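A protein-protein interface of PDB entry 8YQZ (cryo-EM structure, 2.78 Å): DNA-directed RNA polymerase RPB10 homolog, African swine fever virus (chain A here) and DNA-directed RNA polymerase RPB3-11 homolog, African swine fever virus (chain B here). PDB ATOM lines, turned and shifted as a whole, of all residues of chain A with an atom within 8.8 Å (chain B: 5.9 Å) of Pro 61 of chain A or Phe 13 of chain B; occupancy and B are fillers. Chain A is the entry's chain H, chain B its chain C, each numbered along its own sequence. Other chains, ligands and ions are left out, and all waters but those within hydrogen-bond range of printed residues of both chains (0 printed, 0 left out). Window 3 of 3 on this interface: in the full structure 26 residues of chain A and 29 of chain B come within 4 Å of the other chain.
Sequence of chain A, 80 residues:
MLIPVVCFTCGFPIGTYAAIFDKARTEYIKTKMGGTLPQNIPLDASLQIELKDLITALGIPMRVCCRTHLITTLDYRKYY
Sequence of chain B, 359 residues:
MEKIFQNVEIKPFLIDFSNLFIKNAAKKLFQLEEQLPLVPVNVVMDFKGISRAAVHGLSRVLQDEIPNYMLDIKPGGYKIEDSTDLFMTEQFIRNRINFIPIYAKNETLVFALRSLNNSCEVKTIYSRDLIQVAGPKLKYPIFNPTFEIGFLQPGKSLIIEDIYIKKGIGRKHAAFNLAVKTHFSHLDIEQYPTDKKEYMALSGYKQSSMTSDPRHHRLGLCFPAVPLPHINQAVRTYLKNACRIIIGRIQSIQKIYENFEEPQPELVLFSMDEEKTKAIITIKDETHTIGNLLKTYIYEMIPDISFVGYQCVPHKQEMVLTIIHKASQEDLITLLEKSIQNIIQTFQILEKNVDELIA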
ATOM      1  N   CYS A  10      22.056   7.494  -4.515  1.00  0.00           N
ATOM      2  CA  CYS A  10      21.991   8.627  -5.417  1.00  0.00           C
ATOM      3  C   CYS A  10      23.327   9.036  -6.011  1.00  0.00           C
ATOM      4  O   CYS A  10      23.337   9.638  -7.086  1.00  0.00           O
ATOM      5  CB  CYS A  10      21.372   9.837  -4.708  1.00  0.00           C
ATOM      6  SG  CYS A  10      22.377  10.639  -3.495  1.00  0.00           S
ATOM      7  N   PHE A  12      25.667  11.021  -4.398  1.00  0.00           N
ATOM      8  CA  PHE A  12      26.230  12.216  -3.798  1.00  0.00           C
ATOM      9  C   PHE A  12      27.524  11.863  -3.069  1.00  0.00           C
ATOM     10  O   PHE A  12      27.595  10.832  -2.399  1.00  0.00           O
ATOM     11  CB  PHE A  12      25.222  12.845  -2.834  1.00  0.00           C
ATOM     12  CG  PHE A  12      25.677  14.132  -2.223  1.00  0.00           C
ATOM     13  CD1 PHE A  12      25.438  15.334  -2.852  1.00  0.00           C
ATOM     14  CD2 PHE A  12      26.345  14.138  -1.015  1.00  0.00           C
ATOM     15  CE1 PHE A  12      25.860  16.507  -2.292  1.00  0.00           C
ATOM     16  CE2 PHE A  12      26.776  15.304  -0.458  1.00  0.00           C
ATOM     17  CZ  PHE A  12      26.527  16.493  -1.095  1.00  0.00           C
ATOM     18  N   PRO A  13      28.562  12.679  -3.179  1.00  0.00           N
ATOM     19  CA  PRO A  13      29.841  12.314  -2.566  1.00  0.00           C
ATOM     20  C   PRO A  13      29.866  12.486  -1.056  1.00  0.00           C
ATOM     21  O   PRO A  13      30.438  13.447  -0.549  1.00  0.00           O
ATOM     22  CB  PRO A  13      30.829  13.260  -3.254  1.00  0.00           C
ATOM     23  CG  PRO A  13      30.018  14.418  -3.628  1.00  0.00           C
ATOM     24  CD  PRO A  13      28.676  13.903  -3.986  1.00  0.00           C
ATOM     25  N   ILE A  14      29.273  11.554  -0.316  1.00  0.00           N
ATOM     26  CA  ILE A  14      29.295  11.664   1.136  1.00  0.00           C
ATOM     27  C   ILE A  14      30.658  11.329   1.712  1.00  0.00           C
ATOM     28  O   ILE A  14      30.894  11.571   2.896  1.00  0.00           O
ATOM     29  CB  ILE A  14      28.239  10.754   1.785  1.00  0.00           C
ATOM     30  CG1 ILE A  14      28.396   9.322   1.291  1.00  0.00           C
ATOM     31  CG2 ILE A  14      26.861  11.256   1.494  1.00  0.00           C
ATOM     32  CD1 ILE A  14      27.878   8.298   2.218  1.00  0.00           C
ATOM     33  N   THR A  16      33.644  12.556   1.057  1.00  0.00           N
ATOM     34  CA  THR A  16      34.588  13.640   1.274  1.00  0.00           C
ATOM     35  C   THR A  16      34.465  14.226   2.671  1.00  0.00           C
ATOM     36  O   THR A  16      35.356  14.964   3.102  1.00  0.00           O
ATOM     37  CB  THR A  16      34.409  14.729   0.211  1.00  0.00           C
ATOM     38  OG1 THR A  16      35.039  15.936   0.641  1.00  0.00           O
ATOM     39  CG2 THR A  16      32.974  14.999  -0.050  1.00  0.00           C
ATOM     40  N   TYR A  17      33.398  13.903   3.394  1.00  0.00           N
ATOM     41  CA  TYR A  17      33.228  14.337   4.769  1.00  0.00           C
ATOM     42  C   TYR A  17      33.247  13.199   5.772  1.00  0.00           C
ATOM     43  O   TYR A  17      32.940  13.430   6.938  1.00  0.00           O
ATOM     44  CB  TYR A  17      31.913  15.096   4.930  1.00  0.00           C
ATOM     45  CG  TYR A  17      31.531  15.954   3.767  1.00  0.00           C
ATOM     46  CD1 TYR A  17      30.568  15.542   2.868  1.00  0.00           C
ATOM     47  CD2 TYR A  17      32.118  17.188   3.576  1.00  0.00           C
ATOM     48  CE1 TYR A  17      30.210  16.326   1.815  1.00  0.00           C
ATOM     49  CE2 TYR A  17      31.766  17.978   2.523  1.00  0.00           C
ATOM     50  CZ  TYR A  17      30.811  17.544   1.648  1.00  0.00           C
ATOM     51  OH  TYR A  17      30.455  18.333   0.592  1.00  0.00           O
ATOM     52  N   LYS A  52      21.492  15.097  13.587  1.00  0.00           N
ATOM     53  CA  LYS A  52      20.915  15.883  12.503  1.00  0.00           C
ATOM     54  C   LYS A  52      21.745  17.121  12.195  1.00  0.00           C
ATOM     55  O   LYS A  52      22.151  17.342  11.049  1.00  0.00           O
ATOM     56  CB  LYS A  52      19.493  16.270  12.892  1.00  0.00           C
ATOM     57  CG  LYS A  52      18.555  16.608  11.781  1.00  0.00           C
ATOM     58  CD  LYS A  52      17.608  17.670  12.289  1.00  0.00           C
ATOM     59  CE  LYS A  52      17.038  18.539  11.200  1.00  0.00           C
ATOM     60  NZ  LYS A  52      15.744  18.008  10.714  1.00  0.00           N
ATOM     61  N   ILE A  55      25.454  16.672  10.830  1.00  0.00           N
ATOM     62  CA  ILE A  55      25.467  16.371   9.406  1.00  0.00           C
ATOM     63  C   ILE A  55      25.085  17.603   8.604  1.00  0.00           C
ATOM     64  O   ILE A  55      25.628  17.846   7.523  1.00  0.00           O
ATOM     65  CB  ILE A  55      24.541  15.183   9.103  1.00  0.00           C
ATOM     66  CG1 ILE A  55      24.986  13.956   9.875  1.00  0.00           C
ATOM     67  CG2 ILE A  55      24.549  14.867   7.639  1.00  0.00           C
ATOM     68  CD1 ILE A  55      23.996  12.857   9.839  1.00  0.00           C
ATOM     69  N   THR A  56      24.144  18.396   9.113  1.00  0.00           N
ATOM     70  CA  THR A  56      23.798  19.631   8.421  1.00  0.00           C
ATOM     71  C   THR A  56      24.994  20.565   8.337  1.00  0.00           C
ATOM     72  O   THR A  56      25.209  21.217   7.313  1.00  0.00           O
ATOM     73  CB  THR A  56      22.638  20.330   9.121  1.00  0.00           C
ATOM     74  OG1 THR A  56      21.547  19.423   9.276  1.00  0.00           O
ATOM     75  CG2 THR A  56      22.168  21.510   8.303  1.00  0.00           C
ATOM     76  N   ALA A  57      25.777  20.652   9.412  1.00  0.00           N
ATOM     77  CA  ALA A  57      26.961  21.499   9.423  1.00  0.00           C
ATOM     78  C   ALA A  57      28.045  20.995   8.489  1.00  0.00           C
ATOM     79  O   ALA A  57      28.842  21.799   8.003  1.00  0.00           O
ATOM     80  CB  ALA A  57      27.518  21.608  10.837  1.00  0.00           C
ATOM     81  N   LEU A  58      28.111  19.690   8.234  1.00  0.00           N
ATOM     82  CA  LEU A  58      29.052  19.221   7.222  1.00  0.00           C
ATOM     83  C   LEU A  58      28.713  19.704   5.817  1.00  0.00           C
ATOM     84  O   LEU A  58      29.566  19.617   4.932  1.00  0.00           O
ATOM     85  CB  LEU A  58      29.117  17.699   7.218  1.00  0.00           C
ATOM     86  CG  LEU A  58      30.044  17.048   8.231  1.00  0.00           C
ATOM     87  CD1 LEU A  58      29.684  15.602   8.323  1.00  0.00           C
ATOM     88  CD2 LEU A  58      31.488  17.220   7.844  1.00  0.00           C
ATOM     89  N   GLY A  59      27.505  20.203   5.587  1.00  0.00           N
ATOM     90  CA  GLY A  59      27.083  20.588   4.260  1.00  0.00           C
ATOM     91  C   GLY A  59      26.360  19.518   3.477  1.00  0.00           C
ATOM     92  O   GLY A  59      26.102  19.711   2.288  1.00  0.00           O
ATOM     93  N   ILE A  60      26.033  18.394   4.099  1.00  0.00           N
ATOM     94  CA  ILE A  60      25.338  17.295   3.440  1.00  0.00           C
ATOM     95  C   ILE A  60      23.845  17.603   3.443  1.00  0.00           C
ATOM     96  O   ILE A  60      23.320  18.074   4.457  1.00  0.00           O
ATOM     97  CB  ILE A  60      25.664  15.963   4.130  1.00  0.00           C
ATOM     98  CG1 ILE A  60      27.127  15.612   3.886  1.00  0.00           C
ATOM     99  CG2 ILE A  60      24.775  14.844   3.637  1.00  0.00           C
ATOM    100  CD1 ILE A  60      27.607  14.458   4.677  1.00  0.00           C
ATOM    101  N   PRO A  61      23.127  17.379   2.340  1.00  0.00           N
ATOM    102  CA  PRO A  61      21.713  17.770   2.288  1.00  0.00           C
ATOM    103  C   PRO A  61      20.809  16.905   3.150  1.00  0.00           C
ATOM    104  O   PRO A  61      21.265  15.969   3.806  1.00  0.00           O
ATOM    105  CB  PRO A  61      21.362  17.611   0.806  1.00  0.00           C
ATOM    106  CG  PRO A  61      22.650  17.484   0.100  1.00  0.00           C
ATOM    107  CD  PRO A  61      23.593  16.866   1.044  1.00  0.00           C
ATOM    108  N   MET A  62      19.507  17.187   3.113  1.00  0.00           N
ATOM    109  CA  MET A  62      18.512  16.482   3.913  1.00  0.00           C
ATOM    110  C   MET A  62      17.959  15.243   3.226  1.00  0.00           C
ATOM    111  O   MET A  62      16.790  14.907   3.415  1.00  0.00           O
ATOM    112  CB  MET A  62      17.374  17.428   4.284  1.00  0.00           C
ATOM    113  CG  MET A  62      17.455  17.905   5.699  1.00  0.00           C
ATOM    114  SD  MET A  62      17.473  16.496   6.802  1.00  0.00           S
ATOM    115  CE  MET A  62      18.120  17.273   8.251  1.00  0.00           C
ATOM    116  N   ARG A  63      18.768  14.560   2.433  1.00  0.00           N
ATOM    117  CA  ARG A  63      18.337  13.367   1.729  1.00  0.00           C
ATOM    118  C   ARG A  63      18.340  12.155   2.649  1.00  0.00           C
ATOM    119  O   ARG A  63      19.246  11.976   3.456  1.00  0.00           O
ATOM    120  CB  ARG A  63      19.250  13.135   0.535  1.00  0.00           C
ATOM    121  CG  ARG A  63      19.460  14.382  -0.277  1.00  0.00           C
ATOM    122  CD  ARG A  63      20.520  14.190  -1.318  1.00  0.00           C
ATOM    123  NE  ARG A  63      20.102  13.256  -2.351  1.00  0.00           N
ATOM    124  CZ  ARG A  63      19.343  13.567  -3.386  1.00  0.00           C
ATOM    125  NH1 ARG A  63      18.877  14.788  -3.559  1.00  0.00           N
ATOM    126  NH2 ARG A  63      19.037  12.626  -4.268  1.00  0.00           N
ATOM    127  N   VAL A  64      17.309  11.320   2.520  1.00  0.00           N
ATOM    128  CA  VAL A  64      17.154  10.161   3.394  1.00  0.00           C
ATOM    129  C   VAL A  64      18.286   9.168   3.178  1.00  0.00           C
ATOM    130  O   VAL A  64      18.855   8.623   4.134  1.00  0.00           O
ATOM    131  CB  VAL A  64      15.779   9.512   3.156  1.00  0.00           C
ATOM    132  CG1 VAL A  64      15.680   8.166   3.836  1.00  0.00           C
ATOM    133  CG2 VAL A  64      14.686  10.414   3.643  1.00  0.00           C
ATOM    134  N   CYS A  65      18.632   8.926   1.919  1.00  0.00           N
ATOM    135  CA  CYS A  65      19.625   7.923   1.567  1.00  0.00           C
ATOM    136  C   CYS A  65      21.018   8.310   2.050  1.00  0.00           C
ATOM    137  O   CYS A  65      21.759   7.475   2.578  1.00  0.00           O
ATOM    138  CB  CYS A  65      19.600   7.726   0.055  1.00  0.00           C
ATOM    139  SG  CYS A  65      19.726   9.254  -0.913  1.00  0.00           S
ATOM    140  N   CYS A  66      21.396   9.569   1.859  1.00  0.00           N
ATOM    141  CA  CYS A  66      22.756   9.986   2.172  1.00  0.00           C
ATOM    142  C   CYS A  66      23.013   9.937   3.664  1.00  0.00           C
ATOM    143  O   CYS A  66      24.067   9.468   4.108  1.00  0.00           O
ATOM    144  CB  CYS A  66      23.003  11.387   1.630  1.00  0.00           C
ATOM    145  SG  CYS A  66      22.741  11.525  -0.125  1.00  0.00           S
ATOM    146  N   ARG A  67      22.056  10.412   4.453  1.00  0.00           N
ATOM    147  CA  ARG A  67      22.195  10.365   5.896  1.00  0.00           C
ATOM    148  C   ARG A  67      22.107   8.944   6.424  1.00  0.00           C
ATOM    149  O   ARG A  67      22.849   8.587   7.343  1.00  0.00           O
ATOM    150  CB  ARG A  67      21.159  11.281   6.523  1.00  0.00           C
ATOM    151  CG  ARG A  67      21.530  12.716   6.304  1.00  0.00           C
ATOM    152  CD  ARG A  67      20.438  13.667   6.623  1.00  0.00           C
ATOM    153  NE  ARG A  67      20.822  15.026   6.271  1.00  0.00           N
ATOM    154  CZ  ARG A  67      21.160  15.961   7.147  1.00  0.00           C
ATOM    155  NH1 ARG A  67      21.157  15.722   8.445  1.00  0.00           N
ATOM    156  NH2 ARG A  67      21.492  17.169   6.708  1.00  0.00           N
ATOM    157  N   THR A  68      21.261   8.108   5.827  1.00  0.00           N
ATOM    158  CA  THR A  68      21.242   6.697   6.193  1.00  0.00           C
ATOM    159  C   THR A  68      22.620   6.064   6.029  1.00  0.00           C
ATOM    160  O   THR A  68      23.146   5.436   6.959  1.00  0.00           O
ATOM    161  CB  THR A  68      20.214   5.967   5.336  1.00  0.00           C
ATOM    162  OG1 THR A  68      18.947   6.607   5.480  1.00  0.00           O
ATOM    163  CG2 THR A  68      20.088   4.542   5.759  1.00  0.00           C
ATOM    164  N   LEU A  70      25.590   7.463   5.643  1.00  0.00           N
ATOM    165  CA  LEU A  70      26.634   8.091   6.439  1.00  0.00           C
ATOM    166  C   LEU A  70      26.548   7.692   7.905  1.00  0.00           C
ATOM    167  O   LEU A  70      27.563   7.665   8.603  1.00  0.00           O
ATOM    168  CB  LEU A  70      26.536   9.603   6.299  1.00  0.00           C
ATOM    169  CG  LEU A  70      27.565  10.453   7.015  1.00  0.00           C
ATOM    170  CD1 LEU A  70      28.877  10.438   6.280  1.00  0.00           C
ATOM    171  CD2 LEU A  70      27.016  11.836   7.122  1.00  0.00           C
ATOM    172  N   LYS B  11      23.677  27.475  -5.919  1.00  0.00           N
ATOM    173  CA  LYS B  11      23.995  27.491  -4.499  1.00  0.00           C
ATOM    174  C   LYS B  11      24.976  26.391  -4.120  1.00  0.00           C
ATOM    175  O   LYS B  11      24.580  25.229  -3.989  1.00  0.00           O
ATOM    176  CB  LYS B  11      22.715  27.351  -3.682  1.00  0.00           C
ATOM    177  CG  LYS B  11      22.746  28.063  -2.356  1.00  0.00           C
ATOM    178  CD  LYS B  11      22.332  29.513  -2.517  1.00  0.00           C
ATOM    179  CE  LYS B  11      21.088  29.654  -3.380  1.00  0.00           C
ATOM    180  NZ  LYS B  11      20.997  31.009  -3.987  1.00  0.00           N
ATOM    181  N   PRO B  12      26.249  26.712  -3.915  1.00  0.00           N
ATOM    182  CA  PRO B  12      27.209  25.692  -3.490  1.00  0.00           C
ATOM    183  C   PRO B  12      26.920  25.171  -2.093  1.00  0.00           C
ATOM    184  O   PRO B  12      26.371  25.863  -1.235  1.00  0.00           O
ATOM    185  CB  PRO B  12      28.549  26.430  -3.538  1.00  0.00           C
ATOM    186  CG  PRO B  12      28.200  27.840  -3.398  1.00  0.00           C
ATOM    187  CD  PRO B  12      26.893  28.021  -4.092  1.00  0.00           C
ATOM    188  N   PHE B  13      27.307  23.920  -1.874  1.00  0.00           N
ATOM    189  CA  PHE B  13      27.209  23.275  -0.569  1.00  0.00           C
ATOM    190  C   PHE B  13      28.521  23.503   0.172  1.00  0.00           C
ATOM    191  O   PHE B  13      29.571  23.010  -0.246  1.00  0.00           O
ATOM    192  CB  PHE B  13      26.920  21.785  -0.716  1.00  0.00           C
ATOM    193  CG  PHE B  13      25.513  21.475  -1.100  1.00  0.00           C
ATOM    194  CD1 PHE B  13      24.464  22.179  -0.560  1.00  0.00           C
ATOM    195  CD2 PHE B  13      25.236  20.467  -1.987  1.00  0.00           C
ATOM    196  CE1 PHE B  13      23.168  21.883  -0.914  1.00  0.00           C
ATOM    197  CE2 PHE B  13      23.948  20.171  -2.336  1.00  0.00           C
ATOM    198  CZ  PHE B  13      22.915  20.873  -1.802  1.00  0.00           C
ATOM    199  N   LEU B  14      28.459  24.238   1.276  1.00  0.00           N
ATOM    200  CA  LEU B  14      29.640  24.680   1.998  1.00  0.00           C
ATOM    201  C   LEU B  14      29.650  24.123   3.413  1.00  0.00           C
ATOM    202  O   LEU B  14      28.613  23.779   3.975  1.00  0.00           O
ATOM    203  CB  LEU B  14      29.707  26.208   2.041  1.00  0.00           C
ATOM    204  CG  LEU B  14      29.759  26.939   0.700  1.00  0.00           C
ATOM    205  CD1 LEU B  14      29.825  28.425   0.935  1.00  0.00           C
ATOM    206  CD2 LEU B  14      30.951  26.488  -0.116  1.00  0.00           C
ATOM    207  N   ILE B  15      30.846  24.037   3.977  1.00  0.00           N
ATOM    208  CA  ILE B  15      31.040  23.567   5.345  1.00  0.00           C
ATOM    209  C   ILE B  15      30.815  24.715   6.315  1.00  0.00           C
ATOM    210  O   ILE B  15      31.259  25.842   6.082  1.00  0.00           O
ATOM    211  CB  ILE B  15      32.446  22.970   5.514  1.00  0.00           C
ATOM    212  CG1 ILE B  15      32.589  21.685   4.704  1.00  0.00           C
ATOM    213  CG2 ILE B  15      32.739  22.703   6.959  1.00  0.00           C
ATOM    214  CD1 ILE B  15      33.963  21.075   4.766  1.00  0.00           C
ATOM    215  N   GLN B  35      37.246  26.468   3.068  1.00  0.00           N
ATOM    216  CA  GLN B  35      36.452  25.524   2.303  1.00  0.00           C
ATOM    217  C   GLN B  35      37.355  24.604   1.491  1.00  0.00           C
ATOM    218  O   GLN B  35      38.552  24.846   1.335  1.00  0.00           O
ATOM    219  CB  GLN B  35      35.472  26.267   1.401  1.00  0.00           C
ATOM    220  CG  GLN B  35      34.548  27.206   2.151  1.00  0.00           C
ATOM    221  CD  GLN B  35      33.630  26.493   3.125  1.00  0.00           C
ATOM    222  OE1 GLN B  35      33.252  25.348   2.909  1.00  0.00           O
ATOM    223  NE2 GLN B  35      33.269  27.169   4.202  1.00  0.00           N
ATOM    224  N   VAL B  39      33.532  21.841  -4.541  1.00  0.00           N
ATOM    225  CA  VAL B  39      32.297  21.801  -3.759  1.00  0.00           C
ATOM    226  C   VAL B  39      31.146  21.287  -4.616  1.00  0.00           C
ATOM    227  O   VAL B  39      31.194  21.408  -5.843  1.00  0.00           O
ATOM    228  CB  VAL B  39      31.961  23.185  -3.173  1.00  0.00           C
ATOM    229  CG1 VAL B  39      33.006  23.607  -2.174  1.00  0.00           C
ATOM    230  CG2 VAL B  39      31.850  24.213  -4.272  1.00  0.00           C
ATOM    231  N   PRO B  40      30.114  20.689  -4.033  1.00  0.00           N
ATOM    232  CA  PRO B  40      28.897  20.424  -4.802  1.00  0.00           C
ATOM    233  C   PRO B  40      28.092  21.694  -5.003  1.00  0.00           C
ATOM    234  O   PRO B  40      28.056  22.577  -4.147  1.00  0.00           O
ATOM    235  CB  PRO B  40      28.134  19.419  -3.932  1.00  0.00           C
ATOM    236  CG  PRO B  40      29.098  18.945  -2.944  1.00  0.00           C
ATOM    237  CD  PRO B  40      30.057  20.049  -2.714  1.00  0.00           C
ATOM    238  N   VAL B  41      27.429  21.780  -6.147  1.00  0.00           N
ATOM    239  CA  VAL B  41      26.655  22.961  -6.500  1.00  0.00           C
ATOM    240  C   VAL B  41      25.244  22.524  -6.848  1.00  0.00           C
ATOM    241  O   VAL B  41      25.058  21.600  -7.641  1.00  0.00           O
ATOM    242  CB  VAL B  41      27.293  23.733  -7.670  1.00  0.00           C
ATOM    243  CG1 VAL B  41      26.370  24.805  -8.154  1.00  0.00           C
ATOM    244  CG2 VAL B  41      28.596  24.346  -7.237  1.00  0.00           C
ATOM    245  N   ASN B  42      24.257  23.181  -6.254  1.00  0.00           N
ATOM    246  CA  ASN B  42      22.855  22.957  -6.571  1.00  0.00           C
ATOM    247  C   ASN B  42      22.377  24.021  -7.549  1.00  0.00           C
ATOM    248  O   ASN B  42      22.528  25.215  -7.292  1.00  0.00           O
ATOM    249  CB  ASN B  42      22.004  22.991  -5.307  1.00  0.00           C
ATOM    250  CG  ASN B  42      20.637  22.416  -5.516  1.00  0.00           C
ATOM    251  OD1 ASN B  42      20.404  21.678  -6.460  1.00  0.00           O
ATOM    252  ND2 ASN B  42      19.709  22.782  -4.654  1.00  0.00           N
ATOM    253  N   CYS B 222      22.045  18.723  -8.833  1.00  0.00           N
ATOM    254  CA  CYS B 222      23.252  18.978  -8.065  1.00  0.00           C
ATOM    255  C   CYS B 222      24.433  18.350  -8.787  1.00  0.00           C
ATOM    256  O   CYS B 222      24.372  17.186  -9.186  1.00  0.00           O
ATOM    257  CB  CYS B 222      23.124  18.426  -6.648  1.00  0.00           C
ATOM    258  SG  CYS B 222      24.514  18.744  -5.564  1.00  0.00           S
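Pro 61 of chain A touches just one residue of chain B: Phe 13. Phe 13 of chain B touches just these residues of chain A: Gly 59 (3.7 Å) and Pro 61 (3.9 Å). No residue of chain A comes within 4 Å of Pro 12 of chain B. Of the printed residues of chain B, Gly 59 of chain A touches Phe 13 (3.7 Å) and Leu 14 (3.6 Å). Of the printed residues of chain A, Leu 14 of chain B touches Gly 59 (3.6 Å). The nearest printed residue of chain B that does not touch Pro 61 of chain A is Cys 222 of chain B (6.1 Å).
N of Phe 13 of chain B is in hydrogen-bond range of O of Pro 40 of chain B, 2.7 Å away. OE1 of Gln 35 of chain B is in hydrogen-bond range of N of Ile 15 of chain B, at 2.9 Å. The guanidinium group (NE) of Arg 67 of chain A lies within hydrogen-bond range of the backbone carbonyl oxygen (O) of Pro 61 of chain A, 2.7 Å away.
Printed residues of chain A that touch a printed residue of chain B: Tyr 17, Ala 57, Leu 58, Gly 59 and Pro 61. Hydrophobic or aromatic side chains of chain B within 4 Å of the printed part of chain A: Phe 13, Ile 15 and Pro 40. Among the printed residues, 6 pairs touch across the chains. Among the printed residues, no Asp or Glu carboxylate lies within 4 Å of a Lys or Arg side-chain nitrogen of the other chain.
OH of Tyr 17 of chain A touches CD of Pro 40 of chain B (3.7 Å). Ala 57 of chain A touches Ile 15 of chain B. CG1 of Ile 15 of chain B touches O of Leu 58 of chain A (3.7 Å). Gly 59 of chain A touches Phe 13 of chain B. CA of Gly 59 of chain A touches O of Leu 14 of chain B (3.6 Å). Pro 61 of chain A touches Phe 13 of chain B.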
